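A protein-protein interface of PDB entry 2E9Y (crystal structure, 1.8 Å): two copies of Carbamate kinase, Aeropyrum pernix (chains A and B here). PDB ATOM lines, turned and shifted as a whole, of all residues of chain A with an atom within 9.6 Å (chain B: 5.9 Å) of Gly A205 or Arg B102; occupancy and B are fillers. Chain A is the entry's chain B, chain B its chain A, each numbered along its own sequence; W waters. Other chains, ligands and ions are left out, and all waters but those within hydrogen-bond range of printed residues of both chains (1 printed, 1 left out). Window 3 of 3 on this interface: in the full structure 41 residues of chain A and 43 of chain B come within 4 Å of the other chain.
Among the printed residues, pairs that only touch across the chains: Val A206 with Glu B99 (3.9 Å) and Val A206 with Arg B102 (3.7 Å).
Hydrophobic or aromatic side chains of chain B that line the printed part of chain A: His B95.
Printed residues of chain A that touch a printed residue of chain B: Arg A116, Gly A205, Val A206 and Leu A207.
Hydrophobic or aromatic side chains of chain A that line the printed part of chain B: Val A206 and Leu A207.
Among the printed residues, 6 pairs touch across the chains.
Among the printed residues, Asp or Glu carboxylates within 4 Å of a Lys or Arg side-chain nitrogen of the other chain: Arg A116 with Glu B98 (2.7 Å).
No position is printed for both chains.
The backbone carbonyl oxygen (O) of Gly A205 is in hydrogen-bond range of the guanidinium group (NH1) of Arg B102 (2.8 Å).
O of Leu A207 is in hydrogen-bond range of NE2 of His B95 (2.8 Å).
A ring nitrogen (ND1) of His B95 sits at hydrogen-bond distance from the guanidinium group (NH1) of Arg A116.
NH2 of Arg A116 is in salt-bridge range of OE1 of Glu B98, 2.7 Å away.
NH2 of Arg A116 lies within salt-bridge range of OD1 of Asp A175, 2.8 Å away.
O of Arg A116 lies within hydrogen-bond range of N of Val A174 (3.0 Å).
The side-chain carboxylate (OE2) of Glu B99 is in salt-bridge range of the guanidinium group (NH2) of Arg B103 (2.9 Å).
Water W1 lies within hydrogen-bond range of the side-chain carboxylate (OE1) of Glu B99, the backbone NH (N) of Leu A207 and the guanidinium group (NH1) of Arg B102.
Of the printed residues of chain B, Gly A205 touches Arg B102.
Arg B102 touches two residues of chain A.
No residue of chain A comes within 4 Å of Leu B101.
No residue of chain A comes within 4 Å of Gly B105.
Printed residues of chain A within 4 Å of Glu B99: Val A206 (3.9 Å).
Of the printed residues of chain B, Leu A207 touches His B95.
Of the printed residues of chain A, His B95 touches Arg A116 and Leu A207.
Of the printed residues of chain B, Arg A116 touches His B95 (2.9 Å) and Glu B98 (2.7 Å).
Printed residues of chain A within 4 Å of Glu B98: Arg A116 (2.7 Å).
Glu B100 touches none of the printed residues of chain A.
Asp A175 touches none of the printed residues of chain B.
The nearest residue of chain A that does not touch Arg B102 is Leu A207 (4.1 Å).
The nearest printed residue of chain B that does not touch Arg A116 is Arg B102 (5.4 Å).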
ATOM      1  N   ARG A 116      17.992 -19.499  26.273  1.00  0.00           N
ATOM      2  CA  ARG A 116      16.588 -19.674  26.622  1.00  0.00           C
ATOM      3  C   ARG A 116      16.288 -21.167  26.731  1.00  0.00           C
ATOM      4  O   ARG A 116      16.878 -21.988  26.022  1.00  0.00           O
ATOM      5  CB  ARG A 116      15.689 -19.054  25.547  1.00  0.00           C
ATOM      6  CG  ARG A 116      15.778 -17.527  25.443  1.00  0.00           C
ATOM      7  CD  ARG A 116      15.247 -17.052  24.098  1.00  0.00           C
ATOM      8  NE  ARG A 116      16.044 -17.616  23.013  1.00  0.00           N
ATOM      9  CZ  ARG A 116      15.763 -17.496  21.722  1.00  0.00           C
ATOM     10  NH1 ARG A 116      14.689 -16.822  21.334  1.00  0.00           N
ATOM     11  NH2 ARG A 116      16.558 -18.058  20.817  1.00  0.00           N
ATOM     12  N   LEU A 118      13.021 -23.972  26.872  1.00  0.00           N
ATOM     13  CA  LEU A 118      11.602 -24.176  26.627  1.00  0.00           C
ATOM     14  C   LEU A 118      10.982 -24.964  27.773  1.00  0.00           C
ATOM     15  O   LEU A 118      11.551 -25.961  28.225  1.00  0.00           O
ATOM     16  CB  LEU A 118      11.407 -24.945  25.314  1.00  0.00           C
ATOM     17  CG  LEU A 118       9.966 -25.272  24.908  1.00  0.00           C
ATOM     18  CD1 LEU A 118       9.235 -23.982  24.536  1.00  0.00           C
ATOM     19  CD2 LEU A 118       9.978 -26.246  23.730  1.00  0.00           C
ATOM     20  N   VAL A 174      16.459 -23.972  23.781  1.00  0.00           N
ATOM     21  CA  VAL A 174      16.205 -23.230  22.551  1.00  0.00           C
ATOM     22  C   VAL A 174      17.472 -22.828  21.807  1.00  0.00           C
ATOM     23  O   VAL A 174      17.551 -22.933  20.581  1.00  0.00           O
ATOM     24  CB  VAL A 174      15.372 -21.962  22.851  1.00  0.00           C
ATOM     25  CG1 VAL A 174      15.043 -21.224  21.555  1.00  0.00           C
ATOM     26  CG2 VAL A 174      14.092 -22.352  23.580  1.00  0.00           C
ATOM     27  N   ASP A 175      18.478 -22.391  22.549  1.00  0.00           N
ATOM     28  CA  ASP A 175      19.712 -21.947  21.928  1.00  0.00           C
ATOM     29  C   ASP A 175      20.799 -23.011  21.852  1.00  0.00           C
ATOM     30  O   ASP A 175      21.979 -22.697  21.753  1.00  0.00           O
ATOM     31  CB  ASP A 175      20.194 -20.696  22.663  1.00  0.00           C
ATOM     32  CG  ASP A 175      19.203 -19.553  22.534  1.00  0.00           C
ATOM     33  OD1 ASP A 175      19.106 -18.988  21.427  1.00  0.00           O
ATOM     34  OD2 ASP A 175      18.501 -19.237  23.520  1.00  0.00           O
ATOM     35  N   VAL A 199      10.783 -19.881  28.328  1.00  0.00           N
ATOM     36  CA  VAL A 199       9.786 -19.448  27.359  1.00  0.00           C
ATOM     37  C   VAL A 199       8.867 -20.627  27.066  1.00  0.00           C
ATOM     38  O   VAL A 199       9.239 -21.781  27.291  1.00  0.00           O
ATOM     39  CB  VAL A 199      10.431 -18.999  26.017  1.00  0.00           C
ATOM     40  CG1 VAL A 199      11.466 -17.910  26.267  1.00  0.00           C
ATOM     41  CG2 VAL A 199      11.072 -20.191  25.310  1.00  0.00           C
ATOM     42  N   VAL A 200       7.669 -20.333  26.570  1.00  0.00           N
ATOM     43  CA  VAL A 200       6.719 -21.383  26.206  1.00  0.00           C
ATOM     44  C   VAL A 200       6.306 -21.177  24.749  1.00  0.00           C
ATOM     45  O   VAL A 200       6.388 -20.065  24.227  1.00  0.00           O
ATOM     46  CB  VAL A 200       5.442 -21.343  27.080  1.00  0.00           C
ATOM     47  CG1 VAL A 200       5.800 -21.552  28.541  1.00  0.00           C
ATOM     48  CG2 VAL A 200       4.714 -20.019  26.887  1.00  0.00           C
ATOM     49  N   GLU A 201       5.867 -22.248  24.097  1.00  0.00           N
ATOM     50  CA  GLU A 201       5.429 -22.158  22.708  1.00  0.00           C
ATOM     51  C   GLU A 201       3.964 -21.737  22.614  1.00  0.00           C
ATOM     52  O   GLU A 201       3.105 -22.295  23.292  1.00  0.00           O
ATOM     53  CB  GLU A 201       5.607 -23.499  21.997  1.00  0.00           C
ATOM     54  CG  GLU A 201       7.042 -23.870  21.715  1.00  0.00           C
ATOM     55  CD  GLU A 201       7.158 -25.034  20.746  1.00  0.00           C
ATOM     56  OE1 GLU A 201       6.721 -26.150  21.097  1.00  0.00           O
ATOM     57  OE2 GLU A 201       7.684 -24.826  19.631  1.00  0.00           O
ATOM     58  N   ARG A 202       3.689 -20.746  21.774  1.00  0.00           N
ATOM     59  CA  ARG A 202       2.328 -20.248  21.575  1.00  0.00           C
ATOM     60  C   ARG A 202       1.917 -20.475  20.120  1.00  0.00           C
ATOM     61  O   ARG A 202       2.722 -20.953  19.317  1.00  0.00           O
ATOM     62  CB  ARG A 202       2.260 -18.758  21.914  1.00  0.00           C
ATOM     63  CG  ARG A 202       2.440 -18.443  23.390  1.00  0.00           C
ATOM     64  CD  ARG A 202       1.376 -19.124  24.234  1.00  0.00           C
ATOM     65  NE  ARG A 202       1.356 -18.604  25.598  1.00  0.00           N
ATOM     66  CZ  ARG A 202       0.542 -19.045  26.551  1.00  0.00           C
ATOM     67  NH1 ARG A 202      -0.321 -20.021  26.292  1.00  0.00           N
ATOM     68  NH2 ARG A 202       0.587 -18.506  27.759  1.00  0.00           N
ATOM     69  N   PRO A 203       0.656 -20.148  19.765  1.00  0.00           N
ATOM     70  CA  PRO A 203       0.169 -20.328  18.392  1.00  0.00           C
ATOM     71  C   PRO A 203       1.223 -19.944  17.365  1.00  0.00           C
ATOM     72  O   PRO A 203       1.724 -18.819  17.367  1.00  0.00           O
ATOM     73  CB  PRO A 203      -1.056 -19.423  18.349  1.00  0.00           C
ATOM     74  CG  PRO A 203      -1.626 -19.617  19.712  1.00  0.00           C
ATOM     75  CD  PRO A 203      -0.394 -19.542  20.607  1.00  0.00           C
ATOM     76  N   GLY A 204       1.548 -20.889  16.488  1.00  0.00           N
ATOM     77  CA  GLY A 204       2.609 -20.641  15.538  1.00  0.00           C
ATOM     78  C   GLY A 204       3.938 -21.068  16.137  1.00  0.00           C
ATOM     79  O   GLY A 204       4.028 -21.975  16.953  1.00  0.00           O
ATOM     80  N   GLY A 205       4.996 -20.392  15.686  1.00  0.00           N
ATOM     81  CA  GLY A 205       6.307 -20.697  16.257  1.00  0.00           C
ATOM     82  C   GLY A 205       6.651 -19.808  17.456  1.00  0.00           C
ATOM     83  O   GLY A 205       7.693 -19.937  18.072  1.00  0.00           O
ATOM     84  N   VAL A 206       5.732 -18.870  17.766  1.00  0.00           N
ATOM     85  CA  VAL A 206       6.030 -17.834  18.755  1.00  0.00           C
ATOM     86  C   VAL A 206       6.417 -18.410  20.123  1.00  0.00           C
ATOM     87  O   VAL A 206       5.754 -19.287  20.661  1.00  0.00           O
ATOM     88  CB  VAL A 206       4.778 -16.966  18.914  1.00  0.00           C
ATOM     89  CG1 VAL A 206       4.993 -15.927  20.008  1.00  0.00           C
ATOM     90  CG2 VAL A 206       4.447 -16.262  17.610  1.00  0.00           C
ATOM     91  N   LEU A 207       7.509 -17.866  20.652  1.00  0.00           N
ATOM     92  CA  LEU A 207       7.998 -18.250  21.971  1.00  0.00           C
ATOM     93  C   LEU A 207       7.680 -17.090  22.908  1.00  0.00           C
ATOM     94  O   LEU A 207       8.059 -15.948  22.649  1.00  0.00           O
ATOM     95  CB  LEU A 207       9.510 -18.506  21.934  1.00  0.00           C
ATOM     96  CG  LEU A 207       9.972 -19.683  21.063  1.00  0.00           C
ATOM     97  CD1 LEU A 207      11.500 -19.785  21.096  1.00  0.00           C
ATOM     98  CD2 LEU A 207       9.341 -20.978  21.569  1.00  0.00           C
ATOM     99  N   GLU A 208       6.971 -17.386  23.989  1.00  0.00           N
ATOM    100  CA  GLU A 208       6.572 -16.369  24.951  1.00  0.00           C
ATOM    101  C   GLU A 208       7.319 -16.485  26.278  1.00  0.00           C
ATOM    102  O   GLU A 208       7.245 -17.509  26.951  1.00  0.00           O
ATOM    103  CB  GLU A 208       5.065 -16.482  25.193  1.00  0.00           C
ATOM    104  CG  GLU A 208       4.509 -15.561  26.259  1.00  0.00           C
ATOM    105  CD  GLU A 208       3.013 -15.755  26.449  1.00  0.00           C
ATOM    106  OE1 GLU A 208       2.258 -15.533  25.479  1.00  0.00           O
ATOM    107  OE2 GLU A 208       2.592 -16.137  27.561  1.00  0.00           O
ATOM    108  N   HIS B  95      15.334 -12.076  20.326  1.00  0.00           N
ATOM    109  CA  HIS B  95      14.055 -12.779  20.341  1.00  0.00           C
ATOM    110  C   HIS B  95      13.097 -12.262  19.262  1.00  0.00           C
ATOM    111  O   HIS B  95      12.449 -13.043  18.562  1.00  0.00           O
ATOM    112  CB  HIS B  95      13.401 -12.633  21.717  1.00  0.00           C
ATOM    113  CG  HIS B  95      12.399 -13.701  22.029  1.00  0.00           C
ATOM    114  ND1 HIS B  95      12.764 -14.966  22.438  1.00  0.00           N
ATOM    115  CD2 HIS B  95      11.047 -13.700  21.972  1.00  0.00           C
ATOM    116  CE1 HIS B  95      11.680 -15.699  22.622  1.00  0.00           C
ATOM    117  NE2 HIS B  95      10.623 -14.953  22.345  1.00  0.00           N
ATOM    118  N   LEU B  97      13.851 -10.480  16.431  1.00  0.00           N
ATOM    119  CA  LEU B  97      14.355 -10.712  15.082  1.00  0.00           C
ATOM    120  C   LEU B  97      14.154 -12.166  14.664  1.00  0.00           C
ATOM    121  O   LEU B  97      13.718 -12.444  13.545  1.00  0.00           O
ATOM    122  CB  LEU B  97      15.835 -10.337  14.999  1.00  0.00           C
ATOM    123  CG  LEU B  97      16.487 -10.471  13.621  1.00  0.00           C
ATOM    124  CD1 LEU B  97      15.621  -9.794  12.559  1.00  0.00           C
ATOM    125  CD2 LEU B  97      17.871  -9.847  13.663  1.00  0.00           C
ATOM    126  N   GLU B  98      14.468 -13.092  15.565  1.00  0.00           N
ATOM    127  CA  GLU B  98      14.290 -14.510  15.279  1.00  0.00           C
ATOM    128  C   GLU B  98      12.823 -14.807  14.967  1.00  0.00           C
ATOM    129  O   GLU B  98      12.515 -15.566  14.049  1.00  0.00           O
ATOM    130  CB  GLU B  98      14.742 -15.357  16.474  1.00  0.00           C
ATOM    131  CG  GLU B  98      16.244 -15.583  16.549  1.00  0.00           C
ATOM    132  CD  GLU B  98      16.660 -16.351  17.793  1.00  0.00           C
ATOM    133  OE1 GLU B  98      15.785 -16.975  18.432  1.00  0.00           O
ATOM    134  OE2 GLU B  98      17.865 -16.342  18.125  1.00  0.00           O
ATOM    135  N   GLU B  99      11.919 -14.201  15.729  1.00  0.00           N
ATOM    136  CA  GLU B  99      10.490 -14.414  15.519  1.00  0.00           C
ATOM    137  C   GLU B  99      10.054 -13.891  14.152  1.00  0.00           C
ATOM    138  O   GLU B  99       9.271 -14.537  13.449  1.00  0.00           O
ATOM    139  CB  GLU B  99       9.691 -13.712  16.614  1.00  0.00           C
ATOM    140  CG  GLU B  99       8.189 -13.909  16.519  1.00  0.00           C
ATOM    141  CD  GLU B  99       7.453 -13.213  17.645  1.00  0.00           C
ATOM    142  OE1 GLU B  99       7.782 -13.479  18.822  1.00  0.00           O
ATOM    143  OE2 GLU B  99       6.550 -12.400  17.355  1.00  0.00           O
ATOM    144  N   GLU B 100      10.567 -12.722  13.778  1.00  0.00           N
ATOM    145  CA  GLU B 100      10.223 -12.118  12.497  1.00  0.00           C
ATOM    146  C   GLU B 100      10.734 -12.955  11.331  1.00  0.00           C
ATOM    147  O   GLU B 100       9.990 -13.235  10.391  1.00  0.00           O
ATOM    148  CB  GLU B 100      10.794 -10.701  12.405  1.00  0.00           C
ATOM    149  CG  GLU B 100      10.439  -9.963  11.119  1.00  0.00           C
ATOM    150  CD  GLU B 100       8.943  -9.919  10.860  1.00  0.00           C
ATOM    151  OE1 GLU B 100       8.186  -9.594  11.799  1.00  0.00           O
ATOM    152  OE2 GLU B 100       8.524 -10.199   9.717  1.00  0.00           O
ATOM    153  N   LEU B 101      11.999 -13.356  11.394  1.00  0.00           N
ATOM    154  CA  LEU B 101      12.588 -14.160  10.331  1.00  0.00           C
ATOM    155  C   LEU B 101      11.842 -15.480  10.183  1.00  0.00           C
ATOM    156  O   LEU B 101      11.657 -15.981   9.074  1.00  0.00           O
ATOM    157  CB  LEU B 101      14.070 -14.416  10.625  1.00  0.00           C
ATOM    158  CG  LEU B 101      14.944 -13.158  10.644  1.00  0.00           C
ATOM    159  CD1 LEU B 101      16.343 -13.498  11.128  1.00  0.00           C
ATOM    160  CD2 LEU B 101      14.994 -12.553   9.250  1.00  0.00           C
ATOM    161  N   ARG B 102      11.410 -16.033  11.312  1.00  0.00           N
ATOM    162  CA  ARG B 102      10.674 -17.292  11.332  1.00  0.00           C
ATOM    163  C   ARG B 102       9.332 -17.098  10.637  1.00  0.00           C
ATOM    164  O   ARG B 102       8.897 -17.939   9.845  1.00  0.00           O
ATOM    165  CB  ARG B 102      10.448 -17.724  12.779  1.00  0.00           C
ATOM    166  CG  ARG B 102       9.768 -19.063  12.959  1.00  0.00           C
ATOM    167  CD  ARG B 102       9.383 -19.219  14.414  1.00  0.00           C
ATOM    168  NE  ARG B 102      10.502 -18.867  15.283  1.00  0.00           N
ATOM    169  CZ  ARG B 102      10.382 -18.214  16.433  1.00  0.00           C
ATOM    170  NH1 ARG B 102       9.186 -17.836  16.867  1.00  0.00           N
ATOM    171  NH2 ARG B 102      11.460 -17.928  17.146  1.00  0.00           N
ATOM    172  N   ARG B 103       8.682 -15.981  10.943  1.00  0.00           N
ATOM    173  CA  ARG B 103       7.392 -15.649  10.352  1.00  0.00           C
ATOM    174  C   ARG B 103       7.533 -15.555   8.833  1.00  0.00           C
ATOM    175  O   ARG B 103       6.555 -15.694   8.098  1.00  0.00           O
ATOM    176  CB  ARG B 103       6.889 -14.317  10.918  1.00  0.00           C
ATOM    177  CG  ARG B 103       5.554 -13.856  10.358  1.00  0.00           C
ATOM    178  CD  ARG B 103       5.046 -12.611  11.071  1.00  0.00           C
ATOM    179  NE  ARG B 103       4.850 -12.840  12.502  1.00  0.00           N
ATOM    180  CZ  ARG B 103       5.651 -12.376  13.459  1.00  0.00           C
ATOM    181  NH1 ARG B 103       6.714 -11.645  13.149  1.00  0.00           N
ATOM    182  NH2 ARG B 103       5.390 -12.650  14.731  1.00  0.00           N
ATOM    183  N   ARG B 104       8.759 -15.326   8.371  1.00  0.00           N
ATOM    184  CA  ARG B 104       9.028 -15.217   6.944  1.00  0.00           C
ATOM    185  C   ARG B 104       9.586 -16.522   6.380  1.00  0.00           C
ATOM    186  O   ARG B 104      10.061 -16.567   5.245  1.00  0.00           O
ATOM    187  CB  ARG B 104      10.006 -14.069   6.680  1.00  0.00           C
ATOM    188  CG  ARG B 104       9.536 -12.731   7.227  1.00  0.00           C
ATOM    189  CD  ARG B 104      10.399 -11.581   6.730  1.00  0.00           C
ATOM    190  NE  ARG B 104       9.984 -10.305   7.310  1.00  0.00           N
ATOM    191  CZ  ARG B 104      10.453  -9.122   6.928  1.00  0.00           C
ATOM    192  NH1 ARG B 104      11.355  -9.048   5.959  1.00  0.00           N
ATOM    193  NH2 ARG B 104      10.024  -8.014   7.518  1.00  0.00           N
ATOM    194  N   GLY B 105       9.529 -17.583   7.179  1.00  0.00           N
ATOM    195  CA  GLY B 105      10.015 -18.876   6.727  1.00  0.00           C
ATOM    196  C   GLY B 105      11.496 -19.125   6.944  1.00  0.00           C
ATOM    197  O   GLY B 105      12.007 -20.185   6.582  1.00  0.00           O
ATOM    198  N   LEU B 106      12.188 -18.153   7.532  1.00  0.00           N
ATOM    199  CA  LEU B 106      13.618 -18.281   7.795  1.00  0.00           C
ATOM    200  C   LEU B 106      13.850 -18.693   9.244  1.00  0.00           C
ATOM    201  O   LEU B 106      13.459 -17.979  10.168  1.00  0.00           O
ATOM    202  CB  LEU B 106      14.332 -16.952   7.532  1.00  0.00           C
ATOM    203  CG  LEU B 106      14.308 -16.364   6.120  1.00  0.00           C
ATOM    204  CD1 LEU B 106      12.884 -16.035   5.711  1.00  0.00           C
ATOM    205  CD2 LEU B 106      15.164 -15.111   6.087  1.00  0.00           C
ATOM    206  N   ASN B 107      14.486 -19.841   9.441  1.00  0.00           N
ATOM    207  CA  ASN B 107      14.760 -20.319  10.789  1.00  0.00           C
ATOM    208  C   ASN B 107      16.237 -20.174  11.129  1.00  0.00           C
ATOM    209  O   ASN B 107      17.053 -21.034  10.794  1.00  0.00           O
ATOM    210  CB  ASN B 107      14.324 -21.779  10.931  1.00  0.00           C
ATOM    211  CG  ASN B 107      12.838 -21.968  10.685  1.00  0.00           C
ATOM    212  OD1 ASN B 107      12.005 -21.283  11.283  1.00  0.00           O
ATOM    213  ND2 ASN B 107      12.497 -22.903   9.805  1.00  0.00           N
HETATM  214  O   HOH W   1       8.935 -15.751  19.242  1.00  0.00           O
